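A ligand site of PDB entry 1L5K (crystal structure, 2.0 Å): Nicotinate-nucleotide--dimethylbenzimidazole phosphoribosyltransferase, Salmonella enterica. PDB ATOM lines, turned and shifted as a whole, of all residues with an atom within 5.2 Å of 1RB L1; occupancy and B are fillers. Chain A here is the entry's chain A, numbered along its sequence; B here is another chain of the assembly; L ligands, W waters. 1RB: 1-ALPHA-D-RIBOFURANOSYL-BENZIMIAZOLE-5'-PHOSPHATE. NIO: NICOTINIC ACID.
The side-chain carboxylate (OE2) of Glu 317 lies within hydrogen-bond range of a nitrogen (N3) of 1RB L1, at 2.5 Å. The backbone NH (N) of Thr 180 lies within hydrogen-bond range of an oxygen (O1P) of 1RB L1, 3.1 Å away. An oxygen (O1P) of 1RB L1 sits at hydrogen-bond distance from the side-chain hydroxyl of Thr 180 (2.6 Å). OE1 of Glu 174 is in hydrogen-bond range of O2' of 1RB L1, at 2.6 Å. The backbone NH (N) of Ala 178 is in hydrogen-bond range of an oxygen (O3P) of 1RB L1. The backbone NH of Ala 203 lies within hydrogen-bond range of an oxygen (O2P) of 1RB L1, at 2.9 Å. N of Gly 176 is in hydrogen-bond range of O3' of 1RB L1 (3.0 Å). O3' of 1RB L1 sits close to O of Gly 176. The side-chain sulfur of Met 177 sits close to an oxygen (O3') of 1RB L1, 3.8 Å away.
The backbone NH (N) of Glu 317 lies within hydrogen-bond range of the side-chain carboxylate (OE2) of Glu 174, 2.9 Å away. OE2 of Glu 317 is in hydrogen-bond range of NE2 of Gln 88 (3.1 Å). The side-chain hydroxyl of Thr 180 sits at hydrogen-bond distance from the side-chain amino group of Lys 213 (2.8 Å). The side-chain carboxylate (OE1) of Glu 174 is in hydrogen-bond range of the side-chain amide nitrogen (ND2) of Asn 179, at 2.9 Å. The backbone carbonyl oxygen (O) of Gly 176 lies close to the side-chain amide oxygen (OD1) of Asn 179 (3.2 Å). The side-chain amide nitrogen (NE2) of Gln 88 lies within hydrogen-bond range of the backbone carbonyl oxygen (O) of Leu 30 of chain B.
O of Leu 315 sits close to N1 of 1RB L1 (3.3 Å). Merely in contact with 1RB L1: Ala 78 (3.6 Å), Ser 80 (3.7 Å), Val 84 (3.6 Å), Gln 88 (3.6 Å), Leu 175 (3.8 Å), Asn 179 (3.0 Å), Gly 202 (3.7 Å) and Pro 32 of chain B (3.6 Å). Hydrophobic or aromatic side chains within 4 Å of 1RB L1: Ala 78, Val 84, Leu 175, Met 177, Ala 203, Leu 315 and Pro 32 of chain B. 16 residues have an atom within 4 Å of 1RB L1: Ala 78, Ser 80, Val 84, Gln 88, Glu 174, Leu 175, Gly 176, Met 177, Ala 178, Asn 179, Thr 180, Gly 202, Ala 203, Leu 315, Glu 317 and Pro 32 of chain B.
Water W1 lies within hydrogen-bond range of O1P of 1RB L1 (2.7 Å), OG1 of Thr 181 (2.9 Å), O of Val 77 (3.0 Å), O of Ala 178 (3.3 Å) and OG1 of Thr 180 (3.4 Å). Water W2 lies within hydrogen-bond range of the backbone carbonyl oxygen (O) of Val 77 (2.7 Å), an oxygen (O2P) of 1RB L1 (2.7 Å) and the side-chain amino group (NZ) of Lys 213 (2.9 Å). Water W3 lies within hydrogen-bond range of O3P of 1RB L1 (2.7 Å) and OG of Ser 80 (2.8 Å). Water W4 lies within hydrogen-bond range of an oxygen (O2P) of 1RB L1 (2.8 Å), the backbone NH of Val 79 (2.8 Å) and the backbone carbonyl oxygen of Ala 203 (3.0 Å).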
ATOM      1  N   VAL A  77      -1.608  17.717 -14.833  1.00  0.00           N
ATOM      2  CA  VAL A  77      -1.317  16.615 -13.911  1.00  0.00           C
ATOM      3  C   VAL A  77      -0.642  15.407 -14.562  1.00  0.00           C
ATOM      4  O   VAL A  77      -0.321  14.427 -13.879  1.00  0.00           O
ATOM      5  CB  VAL A  77      -2.616  16.110 -13.224  1.00  0.00           C
ATOM      6  CG1 VAL A  77      -3.181  17.193 -12.327  1.00  0.00           C
ATOM      7  CG2 VAL A  77      -3.629  15.676 -14.272  1.00  0.00           C
ATOM      8  N   ALA A  78      -0.444  15.460 -15.878  1.00  0.00           N
ATOM      9  CA  ALA A  78       0.187  14.369 -16.623  1.00  0.00           C
ATOM     10  C   ALA A  78       1.213  14.908 -17.619  1.00  0.00           C
ATOM     11  O   ALA A  78       0.962  15.898 -18.307  1.00  0.00           O
ATOM     12  CB  ALA A  78      -0.880  13.566 -17.355  1.00  0.00           C
ATOM     13  N   VAL A  79       2.352  14.245 -17.713  1.00  0.00           N
ATOM     14  CA  VAL A  79       3.425  14.664 -18.602  1.00  0.00           C
ATOM     15  C   VAL A  79       3.393  13.953 -19.971  1.00  0.00           C
ATOM     16  O   VAL A  79       4.150  14.308 -20.873  1.00  0.00           O
ATOM     17  CB  VAL A  79       4.816  14.478 -17.924  1.00  0.00           C
ATOM     18  CG1 VAL A  79       5.104  12.991 -17.735  1.00  0.00           C
ATOM     19  CG2 VAL A  79       5.897  15.148 -18.736  1.00  0.00           C
ATOM     20  N   SER A  80       2.530  12.964 -20.130  1.00  0.00           N
ATOM     21  CA  SER A  80       2.427  12.269 -21.416  1.00  0.00           C
ATOM     22  C   SER A  80       1.452  13.044 -22.302  1.00  0.00           C
ATOM     23  O   SER A  80       0.389  13.460 -21.855  1.00  0.00           O
ATOM     24  CB  SER A  80       1.890  10.841 -21.253  1.00  0.00           C
ATOM     25  OG  SER A  80       2.715  10.039 -20.439  1.00  0.00           O
ATOM     26  N   VAL A  84      -1.111  10.332 -26.871  1.00  0.00           N
ATOM     27  CA  VAL A  84      -0.583   9.002 -26.575  1.00  0.00           C
ATOM     28  C   VAL A  84      -1.683   7.979 -26.276  1.00  0.00           C
ATOM     29  O   VAL A  84      -1.509   6.793 -26.540  1.00  0.00           O
ATOM     30  CB  VAL A  84       0.446   9.052 -25.403  1.00  0.00           C
ATOM     31  CG1 VAL A  84       1.000   7.665 -25.122  1.00  0.00           C
ATOM     32  CG2 VAL A  84       1.587   9.987 -25.748  1.00  0.00           C
ATOM     33  N   GLN A  88      -1.306   4.719 -28.379  1.00  0.00           N
ATOM     34  CA  GLN A  88      -1.054   3.478 -27.674  1.00  0.00           C
ATOM     35  C   GLN A  88      -2.227   2.513 -27.820  1.00  0.00           C
ATOM     36  O   GLN A  88      -2.045   1.277 -27.791  1.00  0.00           O
ATOM     37  CB  GLN A  88      -0.767   3.756 -26.192  1.00  0.00           C
ATOM     38  CG  GLN A  88      -0.287   2.546 -25.429  1.00  0.00           C
ATOM     39  CD  GLN A  88       1.140   2.149 -25.768  1.00  0.00           C
ATOM     40  OE1 GLN A  88       1.617   2.359 -26.886  1.00  0.00           O
ATOM     41  NE2 GLN A  88       1.841   1.576 -24.797  1.00  0.00           N
ATOM     42  N   GLU A 174      -6.382  -0.638 -18.190  1.00  0.00           N
ATOM     43  CA  GLU A 174      -6.792   0.666 -18.699  1.00  0.00           C
ATOM     44  C   GLU A 174      -5.707   1.374 -19.489  1.00  0.00           C
ATOM     45  O   GLU A 174      -4.553   0.923 -19.530  1.00  0.00           O
ATOM     46  CB  GLU A 174      -7.237   1.567 -17.534  1.00  0.00           C
ATOM     47  CG  GLU A 174      -6.307   1.513 -16.317  1.00  0.00           C
ATOM     48  CD  GLU A 174      -4.862   1.799 -16.667  1.00  0.00           C
ATOM     49  OE1 GLU A 174      -4.549   2.919 -17.118  1.00  0.00           O
ATOM     50  OE2 GLU A 174      -4.027   0.887 -16.490  1.00  0.00           O
ATOM     51  N   LEU A 175      -6.086   2.480 -20.103  1.00  0.00           N
ATOM     52  CA  LEU A 175      -5.196   3.308 -20.884  1.00  0.00           C
ATOM     53  C   LEU A 175      -5.849   4.693 -20.959  1.00  0.00           C
ATOM     54  O   LEU A 175      -6.962   4.830 -21.463  1.00  0.00           O
ATOM     55  CB  LEU A 175      -5.045   2.731 -22.291  1.00  0.00           C
ATOM     56  CG  LEU A 175      -3.990   3.386 -23.162  1.00  0.00           C
ATOM     57  CD1 LEU A 175      -2.620   3.227 -22.498  1.00  0.00           C
ATOM     58  CD2 LEU A 175      -3.981   2.757 -24.553  1.00  0.00           C
ATOM     59  N   GLY A 176      -5.168   5.718 -20.440  1.00  0.00           N
ATOM     60  CA  GLY A 176      -5.718   7.059 -20.477  1.00  0.00           C
ATOM     61  C   GLY A 176      -4.825   8.030 -19.735  1.00  0.00           C
ATOM     62  O   GLY A 176      -4.710   7.962 -18.510  1.00  0.00           O
ATOM     63  N   MET A 177      -4.188   8.929 -20.469  1.00  0.00           N
ATOM     64  CA  MET A 177      -3.290   9.885 -19.862  1.00  0.00           C
ATOM     65  C   MET A 177      -4.009  10.717 -18.795  1.00  0.00           C
ATOM     66  O   MET A 177      -5.118  11.222 -19.022  1.00  0.00           O
ATOM     67  CB  MET A 177      -2.666  10.804 -20.918  1.00  0.00           C
ATOM     68  CG  MET A 177      -2.003  10.054 -22.077  1.00  0.00           C
ATOM     69  SD  MET A 177      -0.858   8.737 -21.560  1.00  0.00           S
ATOM     70  CE  MET A 177      -1.639   7.297 -22.278  1.00  0.00           C
ATOM     71  N   ALA A 178      -3.351  10.826 -17.648  1.00  0.00           N
ATOM     72  CA  ALA A 178      -3.844  11.574 -16.497  1.00  0.00           C
ATOM     73  C   ALA A 178      -4.842  10.805 -15.621  1.00  0.00           C
ATOM     74  O   ALA A 178      -5.405  11.371 -14.679  1.00  0.00           O
ATOM     75  CB  ALA A 178      -4.478  12.900 -16.944  1.00  0.00           C
ATOM     76  N   ASN A 179      -5.057   9.509 -15.895  1.00  0.00           N
ATOM     77  CA  ASN A 179      -6.039   8.787 -15.074  1.00  0.00           C
ATOM     78  C   ASN A 179      -5.653   8.454 -13.643  1.00  0.00           C
ATOM     79  O   ASN A 179      -6.498   8.002 -12.870  1.00  0.00           O
ATOM     80  CB  ASN A 179      -6.582   7.531 -15.810  1.00  0.00           C
ATOM     81  CG  ASN A 179      -5.544   6.439 -16.034  1.00  0.00           C
ATOM     82  OD1 ASN A 179      -4.391   6.546 -15.632  1.00  0.00           O
ATOM     83  ND2 ASN A 179      -5.971   5.355 -16.692  1.00  0.00           N
ATOM     84  N   THR A 180      -4.396   8.673 -13.255  1.00  0.00           N
ATOM     85  CA  THR A 180      -4.032   8.394 -11.867  1.00  0.00           C
ATOM     86  C   THR A 180      -4.532   9.527 -10.951  1.00  0.00           C
ATOM     87  O   THR A 180      -4.532   9.394  -9.729  1.00  0.00           O
ATOM     88  CB  THR A 180      -2.490   8.209 -11.676  1.00  0.00           C
ATOM     89  OG1 THR A 180      -1.801   9.414 -12.027  1.00  0.00           O
ATOM     90  CG2 THR A 180      -1.997   7.054 -12.553  1.00  0.00           C
ATOM     91  N   THR A 181      -4.992  10.622 -11.560  1.00  0.00           N
ATOM     92  CA  THR A 181      -5.528  11.745 -10.788  1.00  0.00           C
ATOM     93  C   THR A 181      -6.930  11.388 -10.290  1.00  0.00           C
ATOM     94  O   THR A 181      -7.196  11.421  -9.080  1.00  0.00           O
ATOM     95  CB  THR A 181      -5.519  13.040 -11.622  1.00  0.00           C
ATOM     96  OG1 THR A 181      -4.176  13.499 -11.771  1.00  0.00           O
ATOM     97  CG2 THR A 181      -6.326  14.140 -10.931  1.00  0.00           C
ATOM     98  N   ILE A 201       3.249   9.722  -8.486  1.00  0.00           N
ATOM     99  CA  ILE A 201       3.903  10.270  -9.678  1.00  0.00           C
ATOM    100  C   ILE A 201       3.303   9.780 -10.995  1.00  0.00           C
ATOM    101  O   ILE A 201       3.674  10.263 -12.072  1.00  0.00           O
ATOM    102  CB  ILE A 201       5.413   9.938  -9.639  1.00  0.00           C
ATOM    103  N   GLY A 202       2.394   8.809 -10.921  1.00  0.00           N
ATOM    104  CA  GLY A 202       1.783   8.291 -12.134  1.00  0.00           C
ATOM    105  C   GLY A 202       2.837   7.907 -13.162  1.00  0.00           C
ATOM    106  O   GLY A 202       3.807   7.223 -12.838  1.00  0.00           O
ATOM    107  N   ALA A 203       2.656   8.345 -14.401  1.00  0.00           N
ATOM    108  CA  ALA A 203       3.610   8.038 -15.453  1.00  0.00           C
ATOM    109  C   ALA A 203       4.749   9.063 -15.472  1.00  0.00           C
ATOM    110  O   ALA A 203       4.791   9.965 -16.309  1.00  0.00           O
ATOM    111  CB  ALA A 203       2.904   8.015 -16.817  1.00  0.00           C
ATOM    112  N   LYS A 213      -0.818  18.496  -8.523  1.00  0.00           N
ATOM    113  CA  LYS A 213      -1.697  17.343  -8.659  1.00  0.00           C
ATOM    114  C   LYS A 213      -2.539  17.170  -7.396  1.00  0.00           C
ATOM    115  O   LYS A 213      -3.735  16.907  -7.465  1.00  0.00           O
ATOM    116  CB  LYS A 213      -0.853  16.085  -8.930  1.00  0.00           C
ATOM    117  CG  LYS A 213      -1.655  14.878  -9.376  1.00  0.00           C
ATOM    118  CD  LYS A 213      -0.701  13.779  -9.812  1.00  0.00           C
ATOM    119  CE  LYS A 213      -1.453  12.499 -10.133  1.00  0.00           C
ATOM    120  NZ  LYS A 213      -0.500  11.412 -10.493  1.00  0.00           N
ATOM    121  N   LEU A 266      -4.863   1.950 -10.735  1.00  0.00           N
ATOM    122  CA  LEU A 266      -6.130   2.326 -11.361  1.00  0.00           C
ATOM    123  C   LEU A 266      -7.190   1.272 -11.058  1.00  0.00           C
ATOM    124  O   LEU A 266      -8.341   1.607 -10.752  1.00  0.00           O
ATOM    125  CB  LEU A 266      -5.980   2.471 -12.885  1.00  0.00           C
ATOM    126  CG  LEU A 266      -5.104   3.606 -13.444  1.00  0.00           C
ATOM    127  CD1 LEU A 266      -5.439   4.913 -12.745  1.00  0.00           C
ATOM    128  CD2 LEU A 266      -3.640   3.283 -13.261  1.00  0.00           C
ATOM    129  N   LEU A 315       3.040   0.382 -14.796  1.00  0.00           N
ATOM    130  CA  LEU A 315       2.753   0.624 -16.206  1.00  0.00           C
ATOM    131  C   LEU A 315       1.250   0.667 -16.455  1.00  0.00           C
ATOM    132  O   LEU A 315       0.770   1.483 -17.240  1.00  0.00           O
ATOM    133  CB  LEU A 315       3.359  -0.472 -17.088  1.00  0.00           C
ATOM    134  CG  LEU A 315       2.894  -0.495 -18.555  1.00  0.00           C
ATOM    135  CD1 LEU A 315       3.307   0.791 -19.269  1.00  0.00           C
ATOM    136  CD2 LEU A 315       3.503  -1.708 -19.266  1.00  0.00           C
ATOM    137  N   GLY A 316       0.506  -0.210 -15.793  1.00  0.00           N
ATOM    138  CA  GLY A 316      -0.928  -0.248 -16.023  1.00  0.00           C
ATOM    139  C   GLY A 316      -1.183  -1.129 -17.241  1.00  0.00           C
ATOM    140  O   GLY A 316      -0.415  -2.056 -17.511  1.00  0.00           O
ATOM    141  N   GLU A 317      -2.243  -0.821 -17.982  1.00  0.00           N
ATOM    142  CA  GLU A 317      -2.631  -1.566 -19.186  1.00  0.00           C
ATOM    143  C   GLU A 317      -3.163  -2.966 -18.886  1.00  0.00           C
ATOM    144  O   GLU A 317      -3.677  -3.654 -19.775  1.00  0.00           O
ATOM    145  CB  GLU A 317      -1.460  -1.700 -20.163  1.00  0.00           C
ATOM    146  CG  GLU A 317      -0.837  -0.382 -20.614  1.00  0.00           C
ATOM    147  CD  GLU A 317       0.198  -0.561 -21.711  1.00  0.00           C
ATOM    148  OE1 GLU A 317       0.404  -1.702 -22.165  1.00  0.00           O
ATOM    149  OE2 GLU A 317       0.823   0.442 -22.116  1.00  0.00           O
ATOM    150  N   LEU B  30       8.083   0.799 -25.799  1.00  0.00           N
ATOM    151  CA  LEU B  30       6.783   1.456 -25.800  1.00  0.00           C
ATOM    152  C   LEU B  30       6.168   1.565 -24.401  1.00  0.00           C
ATOM    153  O   LEU B  30       5.155   0.922 -24.106  1.00  0.00           O
ATOM    154  CB  LEU B  30       5.859   0.695 -26.732  1.00  0.00           C
ATOM    155  CG  LEU B  30       4.891   1.454 -27.643  1.00  0.00           C
ATOM    156  CD1 LEU B  30       5.577   2.647 -28.309  1.00  0.00           C
ATOM    157  CD2 LEU B  30       4.378   0.474 -28.692  1.00  0.00           C
ATOM    158  N   LYS B  31       6.765   2.377 -23.543  1.00  0.00           N
ATOM    159  CA  LYS B  31       6.269   2.537 -22.181  1.00  0.00           C
ATOM    160  C   LYS B  31       7.024   3.639 -21.470  1.00  0.00           C
ATOM    161  O   LYS B  31       8.126   4.016 -21.869  1.00  0.00           O
ATOM    162  CB  LYS B  31       6.497   1.243 -21.391  1.00  0.00           C
ATOM    163  CG  LYS B  31       7.978   0.863 -21.317  1.00  0.00           C
ATOM    164  CD  LYS B  31       8.271  -0.275 -20.360  1.00  0.00           C
ATOM    165  CE  LYS B  31       9.721  -0.696 -20.459  1.00  0.00           C
ATOM    166  NZ  LYS B  31      10.665   0.426 -20.169  1.00  0.00           N
ATOM    167  N   PRO B  32       6.445   4.176 -20.387  1.00  0.00           N
ATOM    168  CA  PRO B  32       7.120   5.226 -19.644  1.00  0.00           C
ATOM    169  C   PRO B  32       8.408   4.597 -19.098  1.00  0.00           C
ATOM    170  O   PRO B  32       8.384   3.480 -18.579  1.00  0.00           O
ATOM    171  CB  PRO B  32       6.122   5.562 -18.545  1.00  0.00           C
ATOM    172  CG  PRO B  32       4.804   5.314 -19.217  1.00  0.00           C
ATOM    173  CD  PRO B  32       5.058   4.014 -19.921  1.00  0.00           C
ATOM    174  N   LEU B 348       8.492  10.747 -24.595  1.00  0.00           N
ATOM    175  CA  LEU B 348       8.199  10.807 -23.172  1.00  0.00           C
ATOM    176  C   LEU B 348       9.454  11.195 -22.391  1.00  0.00           C
ATOM    177  O   LEU B 348      10.534  10.662 -22.632  1.00  0.00           O
ATOM    178  CB  LEU B 348       7.690   9.451 -22.676  1.00  0.00           C
ATOM    179  CG  LEU B 348       6.465   8.863 -23.381  1.00  0.00           C
ATOM    180  CD1 LEU B 348       6.204   7.440 -22.886  1.00  0.00           C
ATOM    181  CD2 LEU B 348       5.259   9.746 -23.144  1.00  0.00           C
HETATM  182  N3  1RB L   1       0.794   2.665 -20.886  1.00  0.00           N
HETATM  183  N1  1RB L   1       0.331   4.089 -19.145  1.00  0.00           N
HETATM  184  C2  1RB L   1       0.243   2.832 -19.677  1.00  0.00           C
HETATM  185  C7A 1RB L   1       1.019   4.796 -20.181  1.00  0.00           C
HETATM  186  C3A 1RB L   1       1.301   3.878 -21.255  1.00  0.00           C
HETATM  187  C4  1RB L   1       2.001   4.304 -22.434  1.00  0.00           C
HETATM  188  C5  1RB L   1       2.410   5.639 -22.533  1.00  0.00           C
HETATM  189  C6  1RB L   1       2.139   6.579 -21.463  1.00  0.00           C
HETATM  190  C7  1RB L   1       1.448   6.170 -20.296  1.00  0.00           C
HETATM  191  P   1RB L   1      -0.655   9.555 -15.486  1.00  0.00           P
HETATM  192  O1P 1RB L   1      -1.805   9.853 -14.569  1.00  0.00           O
HETATM  193  O2P 1RB L   1       0.582  10.231 -14.995  1.00  0.00           O
HETATM  194  O3P 1RB L   1      -0.978  10.045 -16.859  1.00  0.00           O
HETATM  195  O5' 1RB L   1      -0.406   7.970 -15.540  1.00  0.00           O
HETATM  196  C5' 1RB L   1      -1.444   7.092 -15.964  1.00  0.00           C
HETATM  197  C4' 1RB L   1      -1.200   6.727 -17.435  1.00  0.00           C
HETATM  198  O4' 1RB L   1       0.058   5.988 -17.615  1.00  0.00           O
HETATM  199  C3' 1RB L   1      -2.238   5.802 -18.043  1.00  0.00           C
HETATM  200  O3' 1RB L   1      -2.303   5.921 -19.487  1.00  0.00           O
HETATM  201  C2' 1RB L   1      -1.697   4.463 -17.613  1.00  0.00           C
HETATM  202  O2' 1RB L   1      -2.323   3.428 -18.372  1.00  0.00           O
HETATM  203  C1' 1RB L   1      -0.201   4.594 -17.798  1.00  0.00           C
HETATM  204  N   NIO L   2       0.166   4.023 -14.511  1.00  0.00           N
HETATM  205  C1  NIO L   2      -0.377   2.851 -14.021  1.00  0.00           C
HETATM  206  C2  NIO L   2      -0.052   2.491 -12.684  1.00  0.00           C
HETATM  207  C3  NIO L   2       0.834   3.322 -11.864  1.00  0.00           C
HETATM  208  C4  NIO L   2       1.311   4.494 -12.501  1.00  0.00           C
HETATM  209  C5  NIO L   2       1.032   4.901 -13.802  1.00  0.00           C
HETATM  210  C6  NIO L   2      -0.628   1.197 -12.087  1.00  0.00           C
HETATM  211  O1  NIO L   2      -0.338   0.880 -10.905  1.00  0.00           O
HETATM  212  O2  NIO L   2      -1.396   0.453 -12.776  1.00  0.00           O
HETATM  213  O   HOH W   1      -2.403  12.317 -13.684  1.00  0.00           O
HETATM  214  O   HOH W   2       0.796  12.113 -13.027  1.00  0.00           O
HETATM  215  O   HOH W   3       1.135  11.013 -18.321  1.00  0.00           O
HETATM  216  O   HOH W   4       2.441  11.840 -16.262  1.00  0.00           O
